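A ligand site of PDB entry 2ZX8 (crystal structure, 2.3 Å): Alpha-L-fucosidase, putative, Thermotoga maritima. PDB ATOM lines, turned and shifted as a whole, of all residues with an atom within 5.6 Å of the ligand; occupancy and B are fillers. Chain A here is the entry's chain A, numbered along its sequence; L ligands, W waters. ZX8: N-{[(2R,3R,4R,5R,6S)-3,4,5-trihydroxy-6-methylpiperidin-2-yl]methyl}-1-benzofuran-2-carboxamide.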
ATOM      1  N   PHE A  32     -16.119   5.549  17.305  1.00  0.00           N
ATOM      2  CA  PHE A  32     -16.102   4.485  18.299  1.00  0.00           C
ATOM      3  C   PHE A  32     -14.745   3.789  18.095  1.00  0.00           C
ATOM      4  O   PHE A  32     -14.248   3.676  16.964  1.00  0.00           O
ATOM      5  CB  PHE A  32     -17.178   3.449  17.958  1.00  0.00           C
ATOM      6  CG  PHE A  32     -17.972   2.933  19.133  1.00  0.00           C
ATOM      7  CD1 PHE A  32     -17.602   3.235  20.453  1.00  0.00           C
ATOM      8  CD2 PHE A  32     -19.115   2.177  18.896  1.00  0.00           C
ATOM      9  CE1 PHE A  32     -18.409   2.760  21.562  1.00  0.00           C
ATOM     10  CE2 PHE A  32     -19.930   1.701  19.944  1.00  0.00           C
ATOM     11  CZ  PHE A  32     -19.584   1.982  21.290  1.00  0.00           C
ATOM     12  N   HIS A  34     -13.063   0.108  19.246  1.00  0.00           N
ATOM     13  CA  HIS A  34     -12.985  -1.177  19.941  1.00  0.00           C
ATOM     14  C   HIS A  34     -11.559  -1.666  19.717  1.00  0.00           C
ATOM     15  O   HIS A  34     -11.178  -2.105  18.619  1.00  0.00           O
ATOM     16  CB  HIS A  34     -14.010  -2.190  19.384  1.00  0.00           C
ATOM     17  CG  HIS A  34     -15.401  -1.969  19.898  1.00  0.00           C
ATOM     18  ND1 HIS A  34     -16.083  -0.769  19.726  1.00  0.00           N
ATOM     19  CD2 HIS A  34     -16.249  -2.787  20.576  1.00  0.00           C
ATOM     20  CE1 HIS A  34     -17.295  -0.869  20.258  1.00  0.00           C
ATOM     21  NE2 HIS A  34     -17.414  -2.083  20.770  1.00  0.00           N
ATOM     22  N   LEU A  50     -25.499  -7.649  12.085  1.00  0.00           N
ATOM     23  CA  LEU A  50     -26.376  -7.964  13.211  1.00  0.00           C
ATOM     24  C   LEU A  50     -27.797  -7.609  12.772  1.00  0.00           C
ATOM     25  O   LEU A  50     -28.045  -6.496  12.228  1.00  0.00           O
ATOM     26  CB  LEU A  50     -26.038  -7.156  14.495  1.00  0.00           C
ATOM     27  CG  LEU A  50     -26.999  -7.401  15.707  1.00  0.00           C
ATOM     28  CD1 LEU A  50     -26.688  -8.776  16.321  1.00  0.00           C
ATOM     29  CD2 LEU A  50     -26.864  -6.351  16.759  1.00  0.00           C
ATOM     30  N   TYR A  64     -18.203 -10.554  15.075  1.00  0.00           N
ATOM     31  CA  TYR A  64     -17.593  -9.542  15.954  1.00  0.00           C
ATOM     32  C   TYR A  64     -16.273 -10.104  16.514  1.00  0.00           C
ATOM     33  O   TYR A  64     -16.244 -10.937  17.447  1.00  0.00           O
ATOM     34  CB  TYR A  64     -18.518  -9.227  17.130  1.00  0.00           C
ATOM     35  CG  TYR A  64     -19.758  -8.376  16.835  1.00  0.00           C
ATOM     36  CD1 TYR A  64     -20.046  -7.908  15.538  1.00  0.00           C
ATOM     37  CD2 TYR A  64     -20.599  -7.985  17.893  1.00  0.00           C
ATOM     38  CE1 TYR A  64     -21.157  -7.062  15.309  1.00  0.00           C
ATOM     39  CE2 TYR A  64     -21.703  -7.163  17.682  1.00  0.00           C
ATOM     40  CZ  TYR A  64     -21.981  -6.694  16.376  1.00  0.00           C
ATOM     41  OH  TYR A  64     -23.056  -5.870  16.196  1.00  0.00           O
ATOM     42  N   GLU A  66     -14.228  -8.906  18.398  1.00  0.00           N
ATOM     43  CA  GLU A  66     -14.012  -8.677  19.802  1.00  0.00           C
ATOM     44  C   GLU A  66     -14.629  -9.748  20.702  1.00  0.00           C
ATOM     45  O   GLU A  66     -14.359  -9.782  21.882  1.00  0.00           O
ATOM     46  CB  GLU A  66     -14.461  -7.252  20.217  1.00  0.00           C
ATOM     47  CG  GLU A  66     -15.977  -6.958  20.239  1.00  0.00           C
ATOM     48  CD  GLU A  66     -16.576  -6.802  18.846  1.00  0.00           C
ATOM     49  OE1 GLU A  66     -17.808  -6.541  18.696  1.00  0.00           O
ATOM     50  OE2 GLU A  66     -15.806  -6.943  17.887  1.00  0.00           O
ATOM     51  N   TRP A  67     -15.415 -10.639  20.142  1.00  0.00           N
ATOM     52  CA  TRP A  67     -16.004 -11.758  20.916  1.00  0.00           C
ATOM     53  C   TRP A  67     -15.117 -13.006  20.799  1.00  0.00           C
ATOM     54  O   TRP A  67     -15.539 -14.125  21.127  1.00  0.00           O
ATOM     55  CB  TRP A  67     -17.437 -12.106  20.425  1.00  0.00           C
ATOM     56  CG  TRP A  67     -18.521 -11.231  20.999  1.00  0.00           C
ATOM     57  CD1 TRP A  67     -18.669  -9.888  20.843  1.00  0.00           C
ATOM     58  CD2 TRP A  67     -19.594 -11.648  21.860  1.00  0.00           C
ATOM     59  NE1 TRP A  67     -19.743  -9.438  21.544  1.00  0.00           N
ATOM     60  CE2 TRP A  67     -20.339 -10.497  22.184  1.00  0.00           C
ATOM     61  CE3 TRP A  67     -20.001 -12.899  22.393  1.00  0.00           C
ATOM     62  CZ2 TRP A  67     -21.451 -10.528  23.012  1.00  0.00           C
ATOM     63  CZ3 TRP A  67     -21.092 -12.931  23.212  1.00  0.00           C
ATOM     64  CH2 TRP A  67     -21.820 -11.730  23.523  1.00  0.00           C
ATOM     65  N   HIS A 128     -13.846  -4.075  27.517  1.00  0.00           N
ATOM     66  CA  HIS A 128     -14.887  -4.797  26.785  1.00  0.00           C
ATOM     67  C   HIS A 128     -15.314  -6.067  27.547  1.00  0.00           C
ATOM     68  O   HIS A 128     -14.954  -6.262  28.712  1.00  0.00           O
ATOM     69  CB  HIS A 128     -14.423  -5.072  25.380  1.00  0.00           C
ATOM     70  CG  HIS A 128     -15.555  -5.246  24.441  1.00  0.00           C
ATOM     71  ND1 HIS A 128     -16.013  -6.499  24.063  1.00  0.00           N
ATOM     72  CD2 HIS A 128     -16.395  -4.347  23.870  1.00  0.00           C
ATOM     73  CE1 HIS A 128     -17.087  -6.346  23.292  1.00  0.00           C
ATOM     74  NE2 HIS A 128     -17.335  -5.056  23.164  1.00  0.00           N
ATOM     75  N   HIS A 129     -16.096  -6.939  26.920  1.00  0.00           N
ATOM     76  CA  HIS A 129     -16.582  -8.134  27.639  1.00  0.00           C
ATOM     77  C   HIS A 129     -15.521  -9.037  28.251  1.00  0.00           C
ATOM     78  O   HIS A 129     -15.822  -9.761  29.222  1.00  0.00           O
ATOM     79  CB  HIS A 129     -17.498  -9.023  26.740  1.00  0.00           C
ATOM     80  CG  HIS A 129     -18.529  -8.239  25.992  1.00  0.00           C
ATOM     81  ND1 HIS A 129     -19.018  -7.017  26.449  1.00  0.00           N
ATOM     82  CD2 HIS A 129     -19.146  -8.464  24.800  1.00  0.00           C
ATOM     83  CE1 HIS A 129     -19.894  -6.541  25.578  1.00  0.00           C
ATOM     84  NE2 HIS A 129     -19.995  -7.398  24.573  1.00  0.00           N
ATOM     85  N   TYR A 171     -16.368   3.994  26.763  1.00  0.00           N
ATOM     86  CA  TYR A 171     -17.242   2.856  26.611  1.00  0.00           C
ATOM     87  C   TYR A 171     -16.881   1.909  27.768  1.00  0.00           C
ATOM     88  O   TYR A 171     -15.675   1.727  28.109  1.00  0.00           O
ATOM     89  CB  TYR A 171     -17.047   2.162  25.249  1.00  0.00           C
ATOM     90  CG  TYR A 171     -17.606   0.757  25.189  1.00  0.00           C
ATOM     91  CD1 TYR A 171     -18.731   0.455  24.437  1.00  0.00           C
ATOM     92  CD2 TYR A 171     -16.981  -0.292  25.872  1.00  0.00           C
ATOM     93  CE1 TYR A 171     -19.244  -0.841  24.353  1.00  0.00           C
ATOM     94  CE2 TYR A 171     -17.474  -1.584  25.810  1.00  0.00           C
ATOM     95  CZ  TYR A 171     -18.597  -1.864  25.051  1.00  0.00           C
ATOM     96  OH  TYR A 171     -19.090  -3.150  25.020  1.00  0.00           O
ATOM     97  N   LEU A 176     -21.350  -7.446  30.819  1.00  0.00           N
ATOM     98  CA  LEU A 176     -20.626  -8.706  30.722  1.00  0.00           C
ATOM     99  C   LEU A 176     -19.150  -8.512  31.115  1.00  0.00           C
ATOM    100  O   LEU A 176     -18.564  -7.442  30.849  1.00  0.00           O
ATOM    101  CB  LEU A 176     -20.645  -9.206  29.263  1.00  0.00           C
ATOM    102  CG  LEU A 176     -21.976  -9.514  28.600  1.00  0.00           C
ATOM    103  CD1 LEU A 176     -21.731  -9.876  27.071  1.00  0.00           C
ATOM    104  CD2 LEU A 176     -22.686 -10.702  29.399  1.00  0.00           C
ATOM    105  N   TRP A 222     -20.814   5.564  28.035  1.00  0.00           N
ATOM    106  CA  TRP A 222     -21.505   4.683  27.088  1.00  0.00           C
ATOM    107  C   TRP A 222     -21.378   3.278  27.648  1.00  0.00           C
ATOM    108  O   TRP A 222     -20.328   2.622  27.435  1.00  0.00           O
ATOM    109  CB  TRP A 222     -20.820   4.790  25.733  1.00  0.00           C
ATOM    110  CG  TRP A 222     -21.657   4.562  24.469  1.00  0.00           C
ATOM    111  CD1 TRP A 222     -22.144   5.537  23.602  1.00  0.00           C
ATOM    112  CD2 TRP A 222     -22.059   3.297  23.901  1.00  0.00           C
ATOM    113  NE1 TRP A 222     -22.812   4.955  22.534  1.00  0.00           N
ATOM    114  CE2 TRP A 222     -22.777   3.587  22.681  1.00  0.00           C
ATOM    115  CE3 TRP A 222     -21.897   1.960  24.301  1.00  0.00           C
ATOM    116  CZ2 TRP A 222     -23.296   2.603  21.880  1.00  0.00           C
ATOM    117  CZ3 TRP A 222     -22.426   0.969  23.489  1.00  0.00           C
ATOM    118  CH2 TRP A 222     -23.120   1.294  22.284  1.00  0.00           C
ATOM    119  N   ASP A 224     -22.525  -0.824  28.067  1.00  0.00           N
ATOM    120  CA  ASP A 224     -23.024  -1.777  27.100  1.00  0.00           C
ATOM    121  C   ASP A 224     -23.514  -2.989  27.866  1.00  0.00           C
ATOM    122  O   ASP A 224     -23.055  -3.276  29.013  1.00  0.00           O
ATOM    123  CB  ASP A 224     -21.926  -2.198  26.091  1.00  0.00           C
ATOM    124  CG  ASP A 224     -22.523  -2.691  24.754  1.00  0.00           C
ATOM    125  OD1 ASP A 224     -21.761  -3.179  23.881  1.00  0.00           O
ATOM    126  OD2 ASP A 224     -23.765  -2.588  24.574  1.00  0.00           O
ATOM    127  N   MET A 225     -24.473  -3.675  27.244  1.00  0.00           N
ATOM    128  CA  MET A 225     -25.007  -4.906  27.743  1.00  0.00           C
ATOM    129  C   MET A 225     -25.802  -4.867  29.031  1.00  0.00           C
ATOM    130  O   MET A 225     -25.949  -5.883  29.679  1.00  0.00           O
ATOM    131  CB  MET A 225     -23.846  -5.936  27.860  1.00  0.00           C
ATOM    132  CG  MET A 225     -23.628  -6.671  26.554  1.00  0.00           C
ATOM    133  SD  MET A 225     -24.924  -7.987  26.236  1.00  0.00           S
ATOM    134  CE  MET A 225     -24.530  -8.415  24.524  1.00  0.00           C
ATOM    135  N   GLY A 226     -26.327  -3.720  29.396  1.00  0.00           N
ATOM    136  CA  GLY A 226     -27.125  -3.650  30.607  1.00  0.00           C
ATOM    137  C   GLY A 226     -26.203  -3.483  31.786  1.00  0.00           C
ATOM    138  O   GLY A 226     -24.980  -3.580  31.643  1.00  0.00           O
ATOM    139  N   ASP A 253     -28.420   4.648  26.643  1.00  0.00           N
ATOM    140  CA  ASP A 253     -29.606   3.965  27.100  1.00  0.00           C
ATOM    141  C   ASP A 253     -29.418   2.484  27.340  1.00  0.00           C
ATOM    142  O   ASP A 253     -30.365   1.708  27.212  1.00  0.00           O
ATOM    143  CB  ASP A 253     -30.736   4.163  26.048  1.00  0.00           C
ATOM    144  CG  ASP A 253     -30.471   3.402  24.741  1.00  0.00           C
ATOM    145  OD1 ASP A 253     -31.429   3.004  24.015  1.00  0.00           O
ATOM    146  OD2 ASP A 253     -29.281   3.162  24.407  1.00  0.00           O
ATOM    147  N   ARG A 254     -28.206   2.047  27.678  1.00  0.00           N
ATOM    148  CA  ARG A 254     -27.978   0.621  27.848  1.00  0.00           C
ATOM    149  C   ARG A 254     -27.686   0.213  29.293  1.00  0.00           C
ATOM    150  O   ARG A 254     -26.897  -0.695  29.538  1.00  0.00           O
ATOM    151  CB  ARG A 254     -26.812   0.208  26.944  1.00  0.00           C
ATOM    152  CG  ARG A 254     -27.105   0.359  25.444  1.00  0.00           C
ATOM    153  CD  ARG A 254     -25.990  -0.205  24.569  1.00  0.00           C
ATOM    154  NE  ARG A 254     -26.380   0.013  23.195  1.00  0.00           N
ATOM    155  CZ  ARG A 254     -25.988  -0.710  22.161  1.00  0.00           C
ATOM    156  NH1 ARG A 254     -26.443  -0.414  20.945  1.00  0.00           N
ATOM    157  NH2 ARG A 254     -25.114  -1.689  22.320  1.00  0.00           N
ATOM    158  N   THR A 264     -29.868   4.165  21.488  1.00  0.00           N
ATOM    159  CA  THR A 264     -28.919   3.689  20.505  1.00  0.00           C
ATOM    160  C   THR A 264     -29.527   2.611  19.587  1.00  0.00           C
ATOM    161  O   THR A 264     -30.554   2.028  19.904  1.00  0.00           O
ATOM    162  CB  THR A 264     -27.646   3.127  21.254  1.00  0.00           C
ATOM    163  OG1 THR A 264     -28.047   2.096  22.180  1.00  0.00           O
ATOM    164  CG2 THR A 264     -26.915   4.268  22.045  1.00  0.00           C
ATOM    165  N   ALA A 265     -28.906   2.371  18.446  1.00  0.00           N
ATOM    166  CA  ALA A 265     -29.353   1.349  17.483  1.00  0.00           C
ATOM    167  C   ALA A 265     -28.034   0.754  17.018  1.00  0.00           C
ATOM    168  O   ALA A 265     -27.006   1.471  16.911  1.00  0.00           O
ATOM    169  CB  ALA A 265     -30.100   1.969  16.334  1.00  0.00           C
ATOM    170  N   GLU A 266     -28.047  -0.541  16.758  1.00  0.00           N
ATOM    171  CA  GLU A 266     -26.825  -1.244  16.355  1.00  0.00           C
ATOM    172  C   GLU A 266     -27.117  -2.023  15.037  1.00  0.00           C
ATOM    173  O   GLU A 266     -28.027  -2.875  14.981  1.00  0.00           O
ATOM    174  CB  GLU A 266     -26.377  -2.134  17.534  1.00  0.00           C
ATOM    175  CG  GLU A 266     -25.033  -2.836  17.379  1.00  0.00           C
ATOM    176  CD  GLU A 266     -24.558  -3.492  18.681  1.00  0.00           C
ATOM    177  OE1 GLU A 266     -23.995  -4.591  18.597  1.00  0.00           O
ATOM    178  OE2 GLU A 266     -24.727  -2.898  19.780  1.00  0.00           O
ATOM    179  N   VAL A 269     -30.631  -3.436  14.241  1.00  0.00           N
ATOM    180  CA  VAL A 269     -31.388  -3.427  15.487  1.00  0.00           C
ATOM    181  C   VAL A 269     -31.711  -2.071  16.071  1.00  0.00           C
ATOM    182  O   VAL A 269     -30.815  -1.306  16.478  1.00  0.00           O
ATOM    183  CB  VAL A 269     -30.671  -4.303  16.530  1.00  0.00           C
ATOM    184  CG1 VAL A 269     -31.571  -4.459  17.777  1.00  0.00           C
ATOM    185  CG2 VAL A 269     -30.356  -5.652  15.906  1.00  0.00           C
ATOM    186  N   ASN A 270     -33.019  -1.806  16.110  1.00  0.00           N
ATOM    187  CA  ASN A 270     -33.607  -0.574  16.583  1.00  0.00           C
ATOM    188  C   ASN A 270     -33.347   0.624  15.682  1.00  0.00           C
ATOM    189  O   ASN A 270     -33.359   1.784  16.145  1.00  0.00           O
ATOM    190  CB  ASN A 270     -33.164  -0.225  18.004  1.00  0.00           C
ATOM    191  CG  ASN A 270     -33.669  -1.259  19.046  1.00  0.00           C
ATOM    192  OD1 ASN A 270     -34.805  -1.765  18.983  1.00  0.00           O
ATOM    193  ND2 ASN A 270     -32.814  -1.564  20.029  1.00  0.00           N
ATOM    194  N   THR A 283     -24.872   3.007  15.643  1.00  0.00           N
ATOM    195  CA  THR A 283     -23.493   2.602  15.670  1.00  0.00           C
ATOM    196  C   THR A 283     -23.315   1.309  14.835  1.00  0.00           C
ATOM    197  O   THR A 283     -24.241   0.474  14.750  1.00  0.00           O
ATOM    198  CB  THR A 283     -23.014   2.393  17.121  1.00  0.00           C
ATOM    199  OG1 THR A 283     -21.588   2.275  17.158  1.00  0.00           O
ATOM    200  CG2 THR A 283     -23.618   1.111  17.692  1.00  0.00           C
ATOM    201  N   PHE A 290     -16.496  -4.898  15.261  1.00  0.00           N
ATOM    202  CA  PHE A 290     -16.115  -3.635  15.858  1.00  0.00           C
ATOM    203  C   PHE A 290     -14.598  -3.788  16.067  1.00  0.00           C
ATOM    204  O   PHE A 290     -13.824  -2.922  15.704  1.00  0.00           O
ATOM    205  CB  PHE A 290     -16.867  -3.350  17.160  1.00  0.00           C
ATOM    206  CG  PHE A 290     -18.303  -2.971  16.935  1.00  0.00           C
ATOM    207  CD1 PHE A 290     -19.290  -3.973  16.785  1.00  0.00           C
ATOM    208  CD2 PHE A 290     -18.687  -1.630  16.868  1.00  0.00           C
ATOM    209  CE1 PHE A 290     -20.631  -3.640  16.579  1.00  0.00           C
ATOM    210  CE2 PHE A 290     -20.034  -1.263  16.645  1.00  0.00           C
ATOM    211  CZ  PHE A 290     -21.021  -2.267  16.505  1.00  0.00           C
HETATM  212  CAJ ZX8 L   1     -27.525  -4.014  21.129  1.00  0.00           C
HETATM  213  CAQ ZX8 L   1     -28.453  -3.068  20.963  1.00  0.00           C
HETATM  214  CAH ZX8 L   1     -29.018  -2.514  19.825  1.00  0.00           C
HETATM  215  CAF ZX8 L   1     -29.885  -1.421  19.943  1.00  0.00           C
HETATM  216  CAG ZX8 L   1     -30.189  -0.891  21.188  1.00  0.00           C
HETATM  217  CAI ZX8 L   1     -29.636  -1.454  22.334  1.00  0.00           C
HETATM  218  CAR ZX8 L   1     -28.767  -2.537  22.217  1.00  0.00           C
HETATM  219  OAN ZX8 L   1     -28.006  -3.187  23.130  1.00  0.00           O
HETATM  220  CAP ZX8 L   1     -27.233  -4.076  22.428  1.00  0.00           C
HETATM  221  CAO ZX8 L   1     -25.958  -4.659  23.032  1.00  0.00           C
HETATM  222  OAB ZX8 L   1     -25.904  -4.861  24.241  1.00  0.00           O
HETATM  223  NAL ZX8 L   1     -24.936  -4.847  22.181  1.00  0.00           N
HETATM  224  CAK ZX8 L   1     -23.637  -5.370  22.623  1.00  0.00           C
HETATM  225  CAT ZX8 L   1     -22.559  -5.120  21.559  1.00  0.00           C
HETATM  226  NAM ZX8 L   1     -22.330  -3.679  21.374  1.00  0.00           N
HETATM  227  CAS ZX8 L   1     -21.345  -3.446  20.303  1.00  0.00           C
HETATM  228  CAA ZX8 L   1     -21.158  -1.940  20.125  1.00  0.00           C
HETATM  229  CAU ZX8 L   1     -20.002  -4.134  20.575  1.00  0.00           C
HETATM  230  OAC ZX8 L   1     -19.386  -3.612  21.754  1.00  0.00           O
HETATM  231  CAW ZX8 L   1     -20.249  -5.627  20.782  1.00  0.00           C
HETATM  232  OAE ZX8 L   1     -19.040  -6.325  21.106  1.00  0.00           O
HETATM  233  CAV ZX8 L   1     -21.235  -5.770  21.945  1.00  0.00           C
HETATM  234  OAD ZX8 L   1     -21.410  -7.162  22.240  1.00  0.00           O
HETATM  235  O   HOH W   1     -31.817   0.817  22.964  1.00  0.00           O
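NAM of the ligand lies within salt-bridge range of OD1 of Asp 224, 2.6 Å away. The side-chain carboxylate (OE1) of Glu 66 is in hydrogen-bond range of an oxygen (OAE) of the ligand. OAN of the ligand lies close to NH2 of Arg 254 (3.4 Å). A ring nitrogen (NE2) of His 34 is in hydrogen-bond range of an oxygen (OAC) of the ligand (2.7 Å). The side-chain carboxylate of Glu 266 lies within salt-bridge range of a nitrogen (NAM) of the ligand (3.0 Å). The indole nitrogen (NE1) of Trp 67 lies within hydrogen-bond range of an oxygen (OAD) of the ligand, 2.9 Å away. OH of Tyr 171 sits at hydrogen-bond distance from OAC of the ligand. NE2 of His 128 sits at hydrogen-bond distance from OAC of the ligand (2.9 Å). OAD of the ligand sits at hydrogen-bond distance from NE2 of His 129 (2.7 Å).
The side-chain carboxylate (OE2) of Glu 266 is in salt-bridge range of the guanidinium group (NH2) of Arg 254, at 2.8 Å. OD2 of Asp 224 lies within salt-bridge range of NH2 of Arg 254 (2.8 Å). The side-chain carboxylate (OE1) of Glu 266 lies within hydrogen-bond range of the side-chain hydroxyl (OH) of Tyr 64. The side-chain hydroxyl of Thr 264 lies within hydrogen-bond range of the side-chain carboxylate of Asp 253 (2.8 Å). The backbone NH (N) of Thr 283 lies within hydrogen-bond range of the backbone carbonyl oxygen (O) of Ala 265, at 2.9 Å. OG1 of Thr 264 sits at hydrogen-bond distance from NE of Arg 254 (2.9 Å). The side-chain carboxylate (OE2) of Glu 66 lies within hydrogen-bond range of the backbone NH (N) of Phe 290 (3.4 Å). A ring nitrogen (NE2) of His 128 sits close to the side-chain hydroxyl of Tyr 171 (3.2 Å).
Residues that only touch the ligand: Asn 270 (2.9 Å), Thr 264 (3.2 Å), Met 225 (3.5 Å), Val 269 (3.6 Å), Phe 290 (3.6 Å), Ala 265 (3.7 Å), Tyr 64 (3.7 Å) and Phe 32 (3.8 Å). 17 residues have an atom within 4 Å of the ligand: Phe 32, His 34, Tyr 64, Glu 66, Trp 67, His 128, His 129, Tyr 171, Asp 224, Met 225, Arg 254, Thr 264, Ala 265, Glu 266, Val 269, Asn 270 and Phe 290. The nearest printed residue that does not touch the ligand is Trp 222 (4.4 Å).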
